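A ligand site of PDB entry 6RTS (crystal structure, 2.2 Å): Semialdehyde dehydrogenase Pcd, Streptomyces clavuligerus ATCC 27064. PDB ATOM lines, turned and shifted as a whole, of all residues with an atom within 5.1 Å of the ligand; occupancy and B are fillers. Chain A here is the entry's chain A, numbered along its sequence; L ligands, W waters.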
ATOM      1  N   ILE A 160     -34.518  25.365  20.748  1.00  0.00           N
ATOM      2  CA  ILE A 160     -33.406  24.438  20.889  1.00  0.00           C
ATOM      3  C   ILE A 160     -32.824  24.693  22.271  1.00  0.00           C
ATOM      4  O   ILE A 160     -32.361  25.785  22.552  1.00  0.00           O
ATOM      5  CB  ILE A 160     -32.372  24.597  19.745  1.00  0.00           C
ATOM      6  CG1 ILE A 160     -32.997  24.096  18.430  1.00  0.00           C
ATOM      7  CG2 ILE A 160     -31.125  23.765  20.010  1.00  0.00           C
ATOM      8  CD1 ILE A 160     -32.162  24.391  17.173  1.00  0.00           C
ATOM      9  N   SER A 161     -32.888  23.681  23.132  1.00  0.00           N
ATOM     10  CA  SER A 161     -32.470  23.820  24.522  1.00  0.00           C
ATOM     11  C   SER A 161     -31.288  22.941  24.881  1.00  0.00           C
ATOM     12  O   SER A 161     -30.948  21.997  24.167  1.00  0.00           O
ATOM     13  CB  SER A 161     -33.648  23.557  25.464  1.00  0.00           C
ATOM     14  OG  SER A 161     -34.192  22.285  25.254  1.00  0.00           O
ATOM     15  N   ALA A 162     -30.700  23.268  26.041  1.00  0.00           N
ATOM     16  CA  ALA A 162     -29.503  22.645  26.587  1.00  0.00           C
ATOM     17  C   ALA A 162     -29.832  21.630  27.686  1.00  0.00           C
ATOM     18  O   ALA A 162     -30.990  21.519  28.135  1.00  0.00           O
ATOM     19  CB  ALA A 162     -28.605  23.720  27.146  1.00  0.00           C
ATOM     20  N   PHE A 163     -28.812  20.903  28.128  1.00  0.00           N
ATOM     21  CA  PHE A 163     -29.018  19.843  29.114  1.00  0.00           C
ATOM     22  C   PHE A 163     -29.242  20.391  30.504  1.00  0.00           C
ATOM     23  O   PHE A 163     -29.842  19.722  31.318  1.00  0.00           O
ATOM     24  CB  PHE A 163     -27.818  18.865  29.149  1.00  0.00           C
ATOM     25  CG  PHE A 163     -26.643  19.359  29.951  1.00  0.00           C
ATOM     26  CD1 PHE A 163     -26.600  19.181  31.337  1.00  0.00           C
ATOM     27  CD2 PHE A 163     -25.564  19.990  29.332  1.00  0.00           C
ATOM     28  CE1 PHE A 163     -25.531  19.644  32.076  1.00  0.00           C
ATOM     29  CE2 PHE A 163     -24.483  20.459  30.070  1.00  0.00           C
ATOM     30  CZ  PHE A 163     -24.466  20.284  31.439  1.00  0.00           C
ATOM     31  N   ASN A 164     -28.666  21.560  30.800  1.00  0.00           N
ATOM     32  CA  ASN A 164     -28.536  22.007  32.187  1.00  0.00           C
ATOM     33  C   ASN A 164     -29.822  22.627  32.779  1.00  0.00           C
ATOM     34  O   ASN A 164     -30.044  22.536  33.986  1.00  0.00           O
ATOM     35  CB  ASN A 164     -27.336  22.933  32.343  1.00  0.00           C
ATOM     36  CG  ASN A 164     -27.497  24.255  31.617  1.00  0.00           C
ATOM     37  OD1 ASN A 164     -28.126  24.311  30.588  1.00  0.00           O
ATOM     38  ND2 ASN A 164     -26.892  25.297  32.149  1.00  0.00           N
ATOM     39  N   PHE A 165     -30.649  23.256  31.943  1.00  0.00           N
ATOM     40  CA  PHE A 165     -32.014  23.670  32.321  1.00  0.00           C
ATOM     41  C   PHE A 165     -33.029  23.035  31.384  1.00  0.00           C
ATOM     42  O   PHE A 165     -33.562  23.695  30.473  1.00  0.00           O
ATOM     43  CB  PHE A 165     -32.105  25.195  32.352  1.00  0.00           C
ATOM     44  CG  PHE A 165     -31.500  25.792  33.576  1.00  0.00           C
ATOM     45  CD1 PHE A 165     -30.147  26.071  33.616  1.00  0.00           C
ATOM     46  CD2 PHE A 165     -32.273  26.020  34.699  1.00  0.00           C
ATOM     47  CE1 PHE A 165     -29.582  26.593  34.769  1.00  0.00           C
ATOM     48  CE2 PHE A 165     -31.704  26.551  35.848  1.00  0.00           C
ATOM     49  CZ  PHE A 165     -30.361  26.833  35.885  1.00  0.00           C
ATOM     50  N   VAL A 169     -36.042  26.572  30.360  1.00  0.00           N
ATOM     51  CA  VAL A 169     -35.729  27.306  29.121  1.00  0.00           C
ATOM     52  C   VAL A 169     -36.858  27.159  28.094  1.00  0.00           C
ATOM     53  O   VAL A 169     -37.354  28.163  27.603  1.00  0.00           O
ATOM     54  CB  VAL A 169     -34.354  26.897  28.558  1.00  0.00           C
ATOM     55  CG1 VAL A 169     -34.164  27.419  27.134  1.00  0.00           C
ATOM     56  CG2 VAL A 169     -33.257  27.406  29.475  1.00  0.00           C
ATOM     57  N   TRP A 172     -39.950  29.137  29.332  1.00  0.00           N
ATOM     58  CA  TRP A 172     -39.844  30.591  29.082  1.00  0.00           C
ATOM     59  C   TRP A 172     -40.318  30.909  27.663  1.00  0.00           C
ATOM     60  O   TRP A 172     -41.113  31.839  27.455  1.00  0.00           O
ATOM     61  CB  TRP A 172     -38.425  31.123  29.217  1.00  0.00           C
ATOM     62  CG  TRP A 172     -37.791  31.020  30.584  1.00  0.00           C
ATOM     63  CD1 TRP A 172     -38.424  30.949  31.770  1.00  0.00           C
ATOM     64  CD2 TRP A 172     -36.380  31.018  30.881  1.00  0.00           C
ATOM     65  NE1 TRP A 172     -37.505  30.875  32.796  1.00  0.00           N
ATOM     66  CE2 TRP A 172     -36.246  30.913  32.279  1.00  0.00           C
ATOM     67  CE3 TRP A 172     -35.222  31.081  30.100  1.00  0.00           C
ATOM     68  CZ2 TRP A 172     -35.009  30.863  32.926  1.00  0.00           C
ATOM     69  CZ3 TRP A 172     -33.986  31.045  30.728  1.00  0.00           C
ATOM     70  CH2 TRP A 172     -33.889  30.941  32.142  1.00  0.00           C
ATOM     71  N   LYS A 187     -36.688  21.110  20.112  1.00  0.00           N
ATOM     72  CA  LYS A 187     -35.616  20.147  19.988  1.00  0.00           C
ATOM     73  C   LYS A 187     -34.816  20.181  21.290  1.00  0.00           C
ATOM     74  O   LYS A 187     -33.911  21.002  21.434  1.00  0.00           O
ATOM     75  CB  LYS A 187     -34.744  20.451  18.756  1.00  0.00           C
ATOM     76  CG  LYS A 187     -34.100  19.241  18.095  1.00  0.00           C
ATOM     77  CD  LYS A 187     -33.200  18.402  19.002  1.00  0.00           C
ATOM     78  CE  LYS A 187     -31.886  19.111  19.297  1.00  0.00           C
ATOM     79  NZ  LYS A 187     -31.025  18.326  20.236  1.00  0.00           N
ATOM     80  N   PRO A 188     -35.138  19.294  22.240  1.00  0.00           N
ATOM     81  CA  PRO A 188     -34.369  19.272  23.497  1.00  0.00           C
ATOM     82  C   PRO A 188     -32.988  18.672  23.316  1.00  0.00           C
ATOM     83  O   PRO A 188     -32.747  17.999  22.332  1.00  0.00           O
ATOM     84  CB  PRO A 188     -35.216  18.397  24.432  1.00  0.00           C
ATOM     85  CG  PRO A 188     -35.995  17.504  23.532  1.00  0.00           C
ATOM     86  CD  PRO A 188     -36.211  18.270  22.243  1.00  0.00           C
ATOM     87  N   SER A 189     -32.070  18.967  24.245  1.00  0.00           N
ATOM     88  CA  SER A 189     -30.783  18.257  24.325  1.00  0.00           C
ATOM     89  C   SER A 189     -30.980  16.725  24.172  1.00  0.00           C
ATOM     90  O   SER A 189     -31.872  16.135  24.817  1.00  0.00           O
ATOM     91  CB  SER A 189     -30.097  18.534  25.669  1.00  0.00           C
ATOM     92  OG  SER A 189     -28.922  17.745  25.862  1.00  0.00           O
ATOM     93  N   GLU A 190     -30.177  16.138  23.296  1.00  0.00           N
ATOM     94  CA  GLU A 190     -30.027  14.693  23.210  1.00  0.00           C
ATOM     95  C   GLU A 190     -29.680  14.007  24.560  1.00  0.00           C
ATOM     96  O   GLU A 190     -29.955  12.829  24.720  1.00  0.00           O
ATOM     97  CB  GLU A 190     -28.987  14.308  22.142  1.00  0.00           C
ATOM     98  CG  GLU A 190     -27.578  14.868  22.329  1.00  0.00           C
ATOM     99  CD  GLU A 190     -27.324  16.184  21.559  1.00  0.00           C
ATOM    100  OE1 GLU A 190     -26.449  16.184  20.666  1.00  0.00           O
ATOM    101  OE2 GLU A 190     -28.009  17.216  21.848  1.00  0.00           O
ATOM    102  N   GLY A 222     -33.678  13.900  19.253  1.00  0.00           N
ATOM    103  CA  GLY A 222     -32.487  13.550  18.473  1.00  0.00           C
ATOM    104  C   GLY A 222     -31.342  14.505  18.718  1.00  0.00           C
ATOM    105  O   GLY A 222     -31.421  15.383  19.576  1.00  0.00           O
ATOM    106  N   ALA A 223     -30.293  14.366  17.911  1.00  0.00           N
ATOM    107  CA  ALA A 223     -29.041  15.094  18.115  1.00  0.00           C
ATOM    108  C   ALA A 223     -29.020  16.459  17.366  1.00  0.00           C
ATOM    109  O   ALA A 223     -30.088  16.979  16.970  1.00  0.00           O
ATOM    110  CB  ALA A 223     -27.862  14.212  17.702  1.00  0.00           C
ATOM    111  N   ALA A 224     -27.828  17.048  17.219  1.00  0.00           N
ATOM    112  CA  ALA A 224     -27.709  18.356  16.589  1.00  0.00           C
ATOM    113  C   ALA A 224     -28.158  18.381  15.093  1.00  0.00           C
ATOM    114  O   ALA A 224     -28.527  19.446  14.593  1.00  0.00           O
ATOM    115  CB  ALA A 224     -26.284  18.895  16.745  1.00  0.00           C
ATOM    116  N   GLY A 227     -31.655  19.311  15.101  1.00  0.00           N
ATOM    117  CA  GLY A 227     -31.615  20.748  15.390  1.00  0.00           C
ATOM    118  C   GLY A 227     -31.389  21.578  14.129  1.00  0.00           C
ATOM    119  O   GLY A 227     -32.036  22.613  13.950  1.00  0.00           O
ATOM    120  N   GLU A 228     -30.495  21.097  13.259  1.00  0.00           N
ATOM    121  CA  GLU A 228     -30.116  21.809  12.033  1.00  0.00           C
ATOM    122  C   GLU A 228     -31.257  21.891  11.030  1.00  0.00           C
ATOM    123  O   GLU A 228     -31.436  22.896  10.369  1.00  0.00           O
ATOM    124  CB  GLU A 228     -28.862  21.181  11.370  1.00  0.00           C
ATOM    125  CG  GLU A 228     -28.147  22.127  10.394  1.00  0.00           C
ATOM    126  CD  GLU A 228     -27.131  21.448   9.458  1.00  0.00           C
ATOM    127  OE1 GLU A 228     -26.487  22.194   8.670  1.00  0.00           O
ATOM    128  OE2 GLU A 228     -26.960  20.210   9.506  1.00  0.00           O
ATOM    129  N   VAL A 231     -33.563  24.576  12.289  1.00  0.00           N
ATOM    130  CA  VAL A 231     -32.918  25.861  11.981  1.00  0.00           C
ATOM    131  C   VAL A 231     -33.090  26.264  10.506  1.00  0.00           C
ATOM    132  O   VAL A 231     -33.311  27.441  10.205  1.00  0.00           O
ATOM    133  CB  VAL A 231     -31.427  25.803  12.382  1.00  0.00           C
ATOM    134  CG1 VAL A 231     -30.627  26.994  11.832  1.00  0.00           C
ATOM    135  CG2 VAL A 231     -31.303  25.738  13.907  1.00  0.00           C
ATOM    136  N   THR A 242     -30.504  27.889  22.738  1.00  0.00           N
ATOM    137  CA  THR A 242     -29.733  27.956  23.958  1.00  0.00           C
ATOM    138  C   THR A 242     -28.615  26.891  23.910  1.00  0.00           C
ATOM    139  O   THR A 242     -28.858  25.727  23.595  1.00  0.00           O
ATOM    140  CB  THR A 242     -30.676  27.778  25.143  1.00  0.00           C
ATOM    141  OG1 THR A 242     -31.555  28.921  25.218  1.00  0.00           O
ATOM    142  CG2 THR A 242     -29.892  27.645  26.428  1.00  0.00           C
ATOM    143  N   GLY A 243     -27.387  27.289  24.220  1.00  0.00           N
ATOM    144  CA  GLY A 243     -26.256  26.362  24.076  1.00  0.00           C
ATOM    145  C   GLY A 243     -24.936  27.074  24.129  1.00  0.00           C
ATOM    146  O   GLY A 243     -24.884  28.251  24.504  1.00  0.00           O
ATOM    147  N   SER A 244     -23.858  26.373  23.736  1.00  0.00           N
ATOM    148  CA  SER A 244     -22.490  26.931  23.755  1.00  0.00           C
ATOM    149  C   SER A 244     -22.354  28.108  22.807  1.00  0.00           C
ATOM    150  O   SER A 244     -23.139  28.256  21.860  1.00  0.00           O
ATOM    151  CB  SER A 244     -21.437  25.876  23.389  1.00  0.00           C
ATOM    152  OG  SER A 244     -21.689  24.654  24.061  1.00  0.00           O
ATOM    153  N   THR A 245     -21.355  28.947  23.075  1.00  0.00           N
ATOM    154  CA  THR A 245     -20.987  30.060  22.196  1.00  0.00           C
ATOM    155  C   THR A 245     -20.654  29.559  20.778  1.00  0.00           C
ATOM    156  O   THR A 245     -21.067  30.192  19.812  1.00  0.00           O
ATOM    157  CB  THR A 245     -19.846  30.929  22.810  1.00  0.00           C
ATOM    158  OG1 THR A 245     -20.384  31.724  23.867  1.00  0.00           O
ATOM    159  CG2 THR A 245     -19.201  31.868  21.779  1.00  0.00           C
ATOM    160  N   MET A 247     -21.941  27.225  19.004  1.00  0.00           N
ATOM    161  CA  MET A 247     -23.149  26.955  18.248  1.00  0.00           C
ATOM    162  C   MET A 247     -23.745  28.211  17.601  1.00  0.00           C
ATOM    163  O   MET A 247     -24.316  28.121  16.512  1.00  0.00           O
ATOM    164  CB  MET A 247     -24.165  26.301  19.180  1.00  0.00           C
ATOM    165  CG  MET A 247     -25.361  25.684  18.476  1.00  0.00           C
ATOM    166  SD  MET A 247     -26.875  25.986  19.370  1.00  0.00           S
ATOM    167  CE  MET A 247     -27.055  27.746  19.142  1.00  0.00           C
ATOM    168  N   ALA A 250     -22.985  28.887  14.045  1.00  0.00           N
ATOM    169  CA  ALA A 250     -23.768  28.033  13.122  1.00  0.00           C
ATOM    170  C   ALA A 250     -25.164  28.638  12.894  1.00  0.00           C
ATOM    171  O   ALA A 250     -25.509  29.024  11.763  1.00  0.00           O
ATOM    172  CB  ALA A 250     -23.870  26.609  13.645  1.00  0.00           C
ATOM    173  N   VAL A 251     -25.926  28.773  13.977  1.00  0.00           N
ATOM    174  CA  VAL A 251     -27.368  29.070  13.907  1.00  0.00           C
ATOM    175  C   VAL A 251     -27.686  30.495  13.441  1.00  0.00           C
ATOM    176  O   VAL A 251     -28.440  30.677  12.493  1.00  0.00           O
ATOM    177  CB  VAL A 251     -28.062  28.773  15.262  1.00  0.00           C
ATOM    178  CG1 VAL A 251     -29.496  29.313  15.292  1.00  0.00           C
ATOM    179  CG2 VAL A 251     -28.035  27.276  15.538  1.00  0.00           C
ATOM    180  N   GLU A 265     -28.875  32.541  23.158  1.00  0.00           N
ATOM    181  CA  GLU A 265     -28.612  32.501  24.581  1.00  0.00           C
ATOM    182  C   GLU A 265     -27.445  31.526  24.747  1.00  0.00           C
ATOM    183  O   GLU A 265     -27.625  30.326  24.867  1.00  0.00           O
ATOM    184  CB  GLU A 265     -29.847  31.961  25.282  1.00  0.00           C
ATOM    185  CG  GLU A 265     -31.023  32.913  25.288  1.00  0.00           C
ATOM    186  CD  GLU A 265     -30.941  33.991  26.369  1.00  0.00           C
ATOM    187  OE1 GLU A 265     -29.937  33.989  27.164  1.00  0.00           O
ATOM    188  OE2 GLU A 265     -31.880  34.832  26.424  1.00  0.00           O
ATOM    189  N   LEU A 266     -26.245  32.082  24.711  1.00  0.00           N
ATOM    190  CA  LEU A 266     -25.058  31.296  24.513  1.00  0.00           C
ATOM    191  C   LEU A 266     -24.228  31.285  25.822  1.00  0.00           C
ATOM    192  O   LEU A 266     -24.797  31.492  26.904  1.00  0.00           O
ATOM    193  CB  LEU A 266     -24.315  31.785  23.260  1.00  0.00           C
ATOM    194  CG  LEU A 266     -25.170  31.802  21.966  1.00  0.00           C
ATOM    195  CD1 LEU A 266     -24.351  32.288  20.776  1.00  0.00           C
ATOM    196  CD2 LEU A 266     -25.761  30.444  21.632  1.00  0.00           C
ATOM    197  N   GLY A 267     -22.936  30.984  25.750  1.00  0.00           N
ATOM    198  CA  GLY A 267     -22.113  30.892  26.952  1.00  0.00           C
ATOM    199  C   GLY A 267     -21.983  32.151  27.805  1.00  0.00           C
ATOM    200  O   GLY A 267     -22.254  33.282  27.358  1.00  0.00           O
ATOM    201  N   GLY A 268     -21.568  31.914  29.041  1.00  0.00           N
ATOM    202  CA  GLY A 268     -21.176  32.963  29.955  1.00  0.00           C
ATOM    203  C   GLY A 268     -19.811  32.688  30.564  1.00  0.00           C
ATOM    204  O   GLY A 268     -19.295  31.555  30.540  1.00  0.00           O
ATOM    205  N   CYS A 299     -25.354  28.634  33.081  1.00  0.00           N
ATOM    206  CA  CYS A 299     -24.760  29.656  32.236  1.00  0.00           C
ATOM    207  C   CYS A 299     -24.415  30.905  33.056  1.00  0.00           C
ATOM    208  O   CYS A 299     -23.514  31.667  32.712  1.00  0.00           O
ATOM    209  CB  CYS A 299     -25.710  30.027  31.113  1.00  0.00           C
ATOM    210  SG  CYS A 299     -24.917  31.034  29.854  1.00  0.00           S
ATOM    211  N   GLU A 399     -14.898  29.808  28.633  1.00  0.00           N
ATOM    212  CA  GLU A 399     -15.888  29.134  29.443  1.00  0.00           C
ATOM    213  C   GLU A 399     -15.511  27.670  29.445  1.00  0.00           C
ATOM    214  O   GLU A 399     -15.627  27.014  28.405  1.00  0.00           O
ATOM    215  CB  GLU A 399     -17.307  29.329  28.867  1.00  0.00           C
ATOM    216  CG  GLU A 399     -18.414  28.620  29.673  1.00  0.00           C
ATOM    217  CD  GLU A 399     -19.754  28.547  28.946  1.00  0.00           C
ATOM    218  OE1 GLU A 399     -19.846  27.795  27.952  1.00  0.00           O
ATOM    219  OE2 GLU A 399     -20.738  29.190  29.400  1.00  0.00           O
ATOM    220  N   PHE A 401     -17.212  24.566  31.160  1.00  0.00           N
ATOM    221  CA  PHE A 401     -18.522  24.307  31.787  1.00  0.00           C
ATOM    222  C   PHE A 401     -18.342  23.337  32.959  1.00  0.00           C
ATOM    223  O   PHE A 401     -18.602  22.160  32.879  1.00  0.00           O
ATOM    224  CB  PHE A 401     -19.573  23.846  30.737  1.00  0.00           C
ATOM    225  CG  PHE A 401     -20.952  24.388  30.996  1.00  0.00           C
ATOM    226  CD1 PHE A 401     -21.164  25.769  31.117  1.00  0.00           C
ATOM    227  CD2 PHE A 401     -22.032  23.548  31.163  1.00  0.00           C
ATOM    228  CE1 PHE A 401     -22.419  26.282  31.404  1.00  0.00           C
ATOM    229  CE2 PHE A 401     -23.303  24.080  31.448  1.00  0.00           C
ATOM    230  CZ  PHE A 401     -23.478  25.451  31.582  1.00  0.00           C
ATOM    231  N   LEU A 427     -22.705  37.807  29.834  1.00  0.00           N
ATOM    232  CA  LEU A 427     -23.994  37.447  30.416  1.00  0.00           C
ATOM    233  C   LEU A 427     -24.261  38.203  31.708  1.00  0.00           C
ATOM    234  O   LEU A 427     -25.112  39.086  31.757  1.00  0.00           O
ATOM    235  CB  LEU A 427     -24.126  35.938  30.575  1.00  0.00           C
ATOM    236  CG  LEU A 427     -25.446  35.386  31.197  1.00  0.00           C
ATOM    237  CD1 LEU A 427     -26.722  35.876  30.523  1.00  0.00           C
ATOM    238  CD2 LEU A 427     -25.396  33.866  31.190  1.00  0.00           C
ATOM    239  N   PHE A 468     -34.012  38.059  30.538  1.00  0.00           N
ATOM    240  CA  PHE A 468     -32.851  37.240  30.780  1.00  0.00           C
ATOM    241  C   PHE A 468     -32.044  37.096  29.490  1.00  0.00           C
ATOM    242  O   PHE A 468     -32.583  36.669  28.464  1.00  0.00           O
ATOM    243  CB  PHE A 468     -33.274  35.874  31.267  1.00  0.00           C
ATOM    244  CG  PHE A 468     -32.121  34.989  31.613  1.00  0.00           C
ATOM    245  CD1 PHE A 468     -31.471  35.128  32.829  1.00  0.00           C
ATOM    246  CD2 PHE A 468     -31.668  34.029  30.709  1.00  0.00           C
ATOM    247  CE1 PHE A 468     -30.405  34.306  33.157  1.00  0.00           C
ATOM    248  CE2 PHE A 468     -30.613  33.196  31.030  1.00  0.00           C
ATOM    249  CZ  PHE A 468     -29.966  33.345  32.264  1.00  0.00           C
ATOM    250  N   THR A 474     -22.252  35.985  24.240  1.00  0.00           N
ATOM    251  CA  THR A 474     -23.495  35.411  24.808  1.00  0.00           C
ATOM    252  C   THR A 474     -24.715  35.478  23.832  1.00  0.00           C
ATOM    253  O   THR A 474     -25.681  34.713  23.980  1.00  0.00           O
ATOM    254  CB  THR A 474     -23.797  36.067  26.159  1.00  0.00           C
ATOM    255  OG1 THR A 474     -22.637  35.955  26.986  1.00  0.00           O
ATOM    256  CG2 THR A 474     -25.004  35.384  26.828  1.00  0.00           C
ATOM    257  N   GLU A 479     -34.939  36.525  27.049  1.00  0.00           N
ATOM    258  CA  GLU A 479     -36.070  35.632  27.361  1.00  0.00           C
ATOM    259  C   GLU A 479     -36.802  36.044  28.636  1.00  0.00           C
ATOM    260  O   GLU A 479     -36.276  36.782  29.456  1.00  0.00           O
ATOM    261  CB  GLU A 479     -35.551  34.209  27.554  1.00  0.00           C
ATOM    262  CG  GLU A 479     -35.155  33.499  26.273  1.00  0.00           C
ATOM    263  CD  GLU A 479     -34.270  32.288  26.513  1.00  0.00           C
ATOM    264  OE1 GLU A 479     -34.430  31.286  25.756  1.00  0.00           O
ATOM    265  OE2 GLU A 479     -33.394  32.354  27.419  1.00  0.00           O
HETATM  266  P1  LIG L   1     -24.794  22.576  23.343  1.00  0.00           P
HETATM  267  O1  LIG L   1     -24.352  23.839  22.651  1.00  0.00           O
HETATM  268  O2  LIG L   1     -23.898  21.372  23.328  1.00  0.00           O
HETATM  269  O3  LIG L   1     -26.209  22.027  22.792  1.00  0.00           O
HETATM  270  C1  LIG L   1     -27.401  22.791  22.989  1.00  0.00           C
HETATM  271  C2  LIG L   1     -28.501  22.349  22.036  1.00  0.00           C
HETATM  272  O4  LIG L   1     -28.201  22.785  20.703  1.00  0.00           O
HETATM  273  C3  LIG L   1     -28.714  20.842  21.948  1.00  0.00           C
HETATM  274  O5  LIG L   1     -30.123  20.588  21.837  1.00  0.00           O
HETATM  275  C4  LIG L   1     -27.944  20.438  20.699  1.00  0.00           C
HETATM  276  O6  LIG L   1     -28.478  19.296  20.039  1.00  0.00           O
HETATM  277  C5  LIG L   1     -28.143  21.669  19.820  1.00  0.00           C
HETATM  278  N1  LIG L   1     -27.094  21.980  18.814  1.00  0.00           N
HETATM  279  C6  LIG L   1     -25.746  21.935  18.937  1.00  0.00           C
HETATM  280  N2  LIG L   1     -25.163  22.345  17.777  1.00  0.00           N
HETATM  281  C7  LIG L   1     -26.152  22.651  16.912  1.00  0.00           C
HETATM  282  C8  LIG L   1     -26.259  23.159  15.519  1.00  0.00           C
HETATM  283  N3  LIG L   1     -25.159  23.416  14.773  1.00  0.00           N
HETATM  284  N4  LIG L   1     -27.495  23.343  15.008  1.00  0.00           N
HETATM  285  C9  LIG L   1     -28.621  23.103  15.717  1.00  0.00           C
HETATM  286  N5  LIG L   1     -28.606  22.656  16.978  1.00  0.00           N
HETATM  287  C10 LIG L   1     -27.422  22.416  17.602  1.00  0.00           C
HETATM  288  O7  LIG L   1     -25.062  23.066  24.849  1.00  0.00           O
HETATM  289  P2  LIG L   1     -25.097  22.104  26.150  1.00  0.00           P
HETATM  290  O8  LIG L   1     -26.300  21.158  26.051  1.00  0.00           O
HETATM  291  O9  LIG L   1     -23.714  21.533  26.439  1.00  0.00           O
HETATM  292  O10 LIG L   1     -25.398  23.267  27.272  1.00  0.00           O
HETATM  293  C11 LIG L   1     -24.445  24.097  27.963  1.00  0.00           C
HETATM  294  C12 LIG L   1     -24.081  25.364  27.184  1.00  0.00           C
HETATM  295  O11 LIG L   1     -25.262  26.160  26.951  1.00  0.00           O
HETATM  296  C13 LIG L   1     -23.120  26.253  27.960  1.00  0.00           C
HETATM  297  O12 LIG L   1     -22.220  26.910  27.085  1.00  0.00           O
HETATM  298  C14 LIG L   1     -24.059  27.260  28.629  1.00  0.00           C
HETATM  299  O13 LIG L   1     -23.496  28.517  29.001  1.00  0.00           O
HETATM  300  C15 LIG L   1     -25.154  27.437  27.594  1.00  0.00           C
HETATM  301  N6  LIG L   1     -26.376  27.883  28.247  1.00  0.00           N
HETATM  302  C16 LIG L   1     -26.811  29.143  28.033  1.00  0.00           C
HETATM  303  C17 LIG L   1     -27.966  29.624  28.645  1.00  0.00           C
HETATM  304  C18 LIG L   1     -28.475  31.023  28.434  1.00  0.00           C
HETATM  305  O14 LIG L   1     -29.666  31.192  28.620  1.00  0.00           O
HETATM  306  N7  LIG L   1     -27.684  32.040  28.034  1.00  0.00           N
HETATM  307  C19 LIG L   1     -28.690  28.759  29.483  1.00  0.00           C
HETATM  308  C20 LIG L   1     -28.242  27.454  29.689  1.00  0.00           C
HETATM  309  C21 LIG L   1     -27.064  27.037  29.059  1.00  0.00           C
HETATM  310  O   HOH W   1     -27.380  24.788  12.710  1.00  0.00           O
HETATM  311  O   HOH W   2     -21.398  22.611  27.697  1.00  0.00           O
HETATM  312  O   HOH W   3     -32.033  30.216  27.689  1.00  0.00           O
HETATM  313  O   HOH W   4     -22.530  23.673  18.153  1.00  0.00           O
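O12 of the ligand lies within hydrogen-bond range of OE1 of Glu 399, at 2.7 Å.
The side-chain amino group of Lys 187 lies within hydrogen-bond range of an oxygen (O6) of the ligand (2.7 Å).
OE2 of Glu 190 is in hydrogen-bond range of O6 of the ligand, 2.8 Å away.
N of Ser 244 is in hydrogen-bond range of O1 of the ligand (2.8 Å).
An oxygen (O1) of the ligand is in hydrogen-bond range of the side-chain hydroxyl of Ser 244 (3.1 Å).
O of Ser 161 lies within hydrogen-bond range of O5 of the ligand, 2.8 Å away.
O13 of the ligand sits at hydrogen-bond distance from SG of Cys 299 (3.0 Å).
OE1 of Glu 265 lies within hydrogen-bond range of N7 of the ligand, at 3.1 Å.
The backbone carbonyl oxygen of Leu 266 sits at hydrogen-bond distance from a nitrogen (N7) of the ligand (3.1 Å).
O8 of the ligand sits at hydrogen-bond distance from N of Phe 163, at 3.3 Å.
N of Ser 189 lies close to O5 of the ligand (3.5 Å).
The side-chain carboxylate (OE2) of Glu 399 is in hydrogen-bond range of the backbone NH (N) of Gly 268 (2.9 Å).
The backbone NH (N) of Ser 161 is in hydrogen-bond range of the backbone carbonyl oxygen (O) of Lys 187 (3.3 Å).
The backbone carbonyl oxygen of Ser 161 is in hydrogen-bond range of the backbone NH of Ser 189.
The side-chain sulfur of Cys 299 sits at hydrogen-bond distance from the backbone NH of Gly 268 (3.6 Å).
The backbone NH of Leu 266 lies within hydrogen-bond range of the backbone carbonyl oxygen of Thr 474.
O of Phe 468 sits at hydrogen-bond distance from N of Glu 479 (2.8 Å).
O of Gly 267 lies within hydrogen-bond range of OG1 of Thr 474.
The backbone NH (N) of Gly 267 sits at hydrogen-bond distance from the side-chain hydroxyl (OG1) of Thr 245, 3.3 Å away.
The backbone carbonyl oxygen (O) of Gly 243 lies close to an oxygen (O11) of the ligand, 3.2 Å away.
SD of Met 247 lies close to O4 of the ligand, 3.7 Å away.
Residues that only touch the ligand: Ile 160 (3.2 Å), Ala 162 (3.2 Å), Asn 164 (3.3 Å), Phe 468 (3.3 Å), Thr 242 (3.3 Å), Phe 401 (3.4 Å), Gly 267 (3.4 Å), Gly 227 (3.5 Å), Ala 250 (3.6 Å), Ala 224 (3.7 Å), Glu 228 (3.7 Å), Pro 188 (3.7 Å), Gly 268 (3.9 Å) and Ala 223 (3.9 Å).
Hydrophobic or aromatic side chains that line the ligand: Ile 160, Ala 162, Phe 163, Ala 224, Met 247, Ala 250, Phe 401 and Phe 468.
The nearest printed residue that does not touch the ligand is Val 251 (4.01 Å).
Water W3 lies within hydrogen-bond range of OE2 of Glu 479 (2.5 Å), O14 of the ligand (2.7 Å) and OG1 of Thr 242 (2.8 Å).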
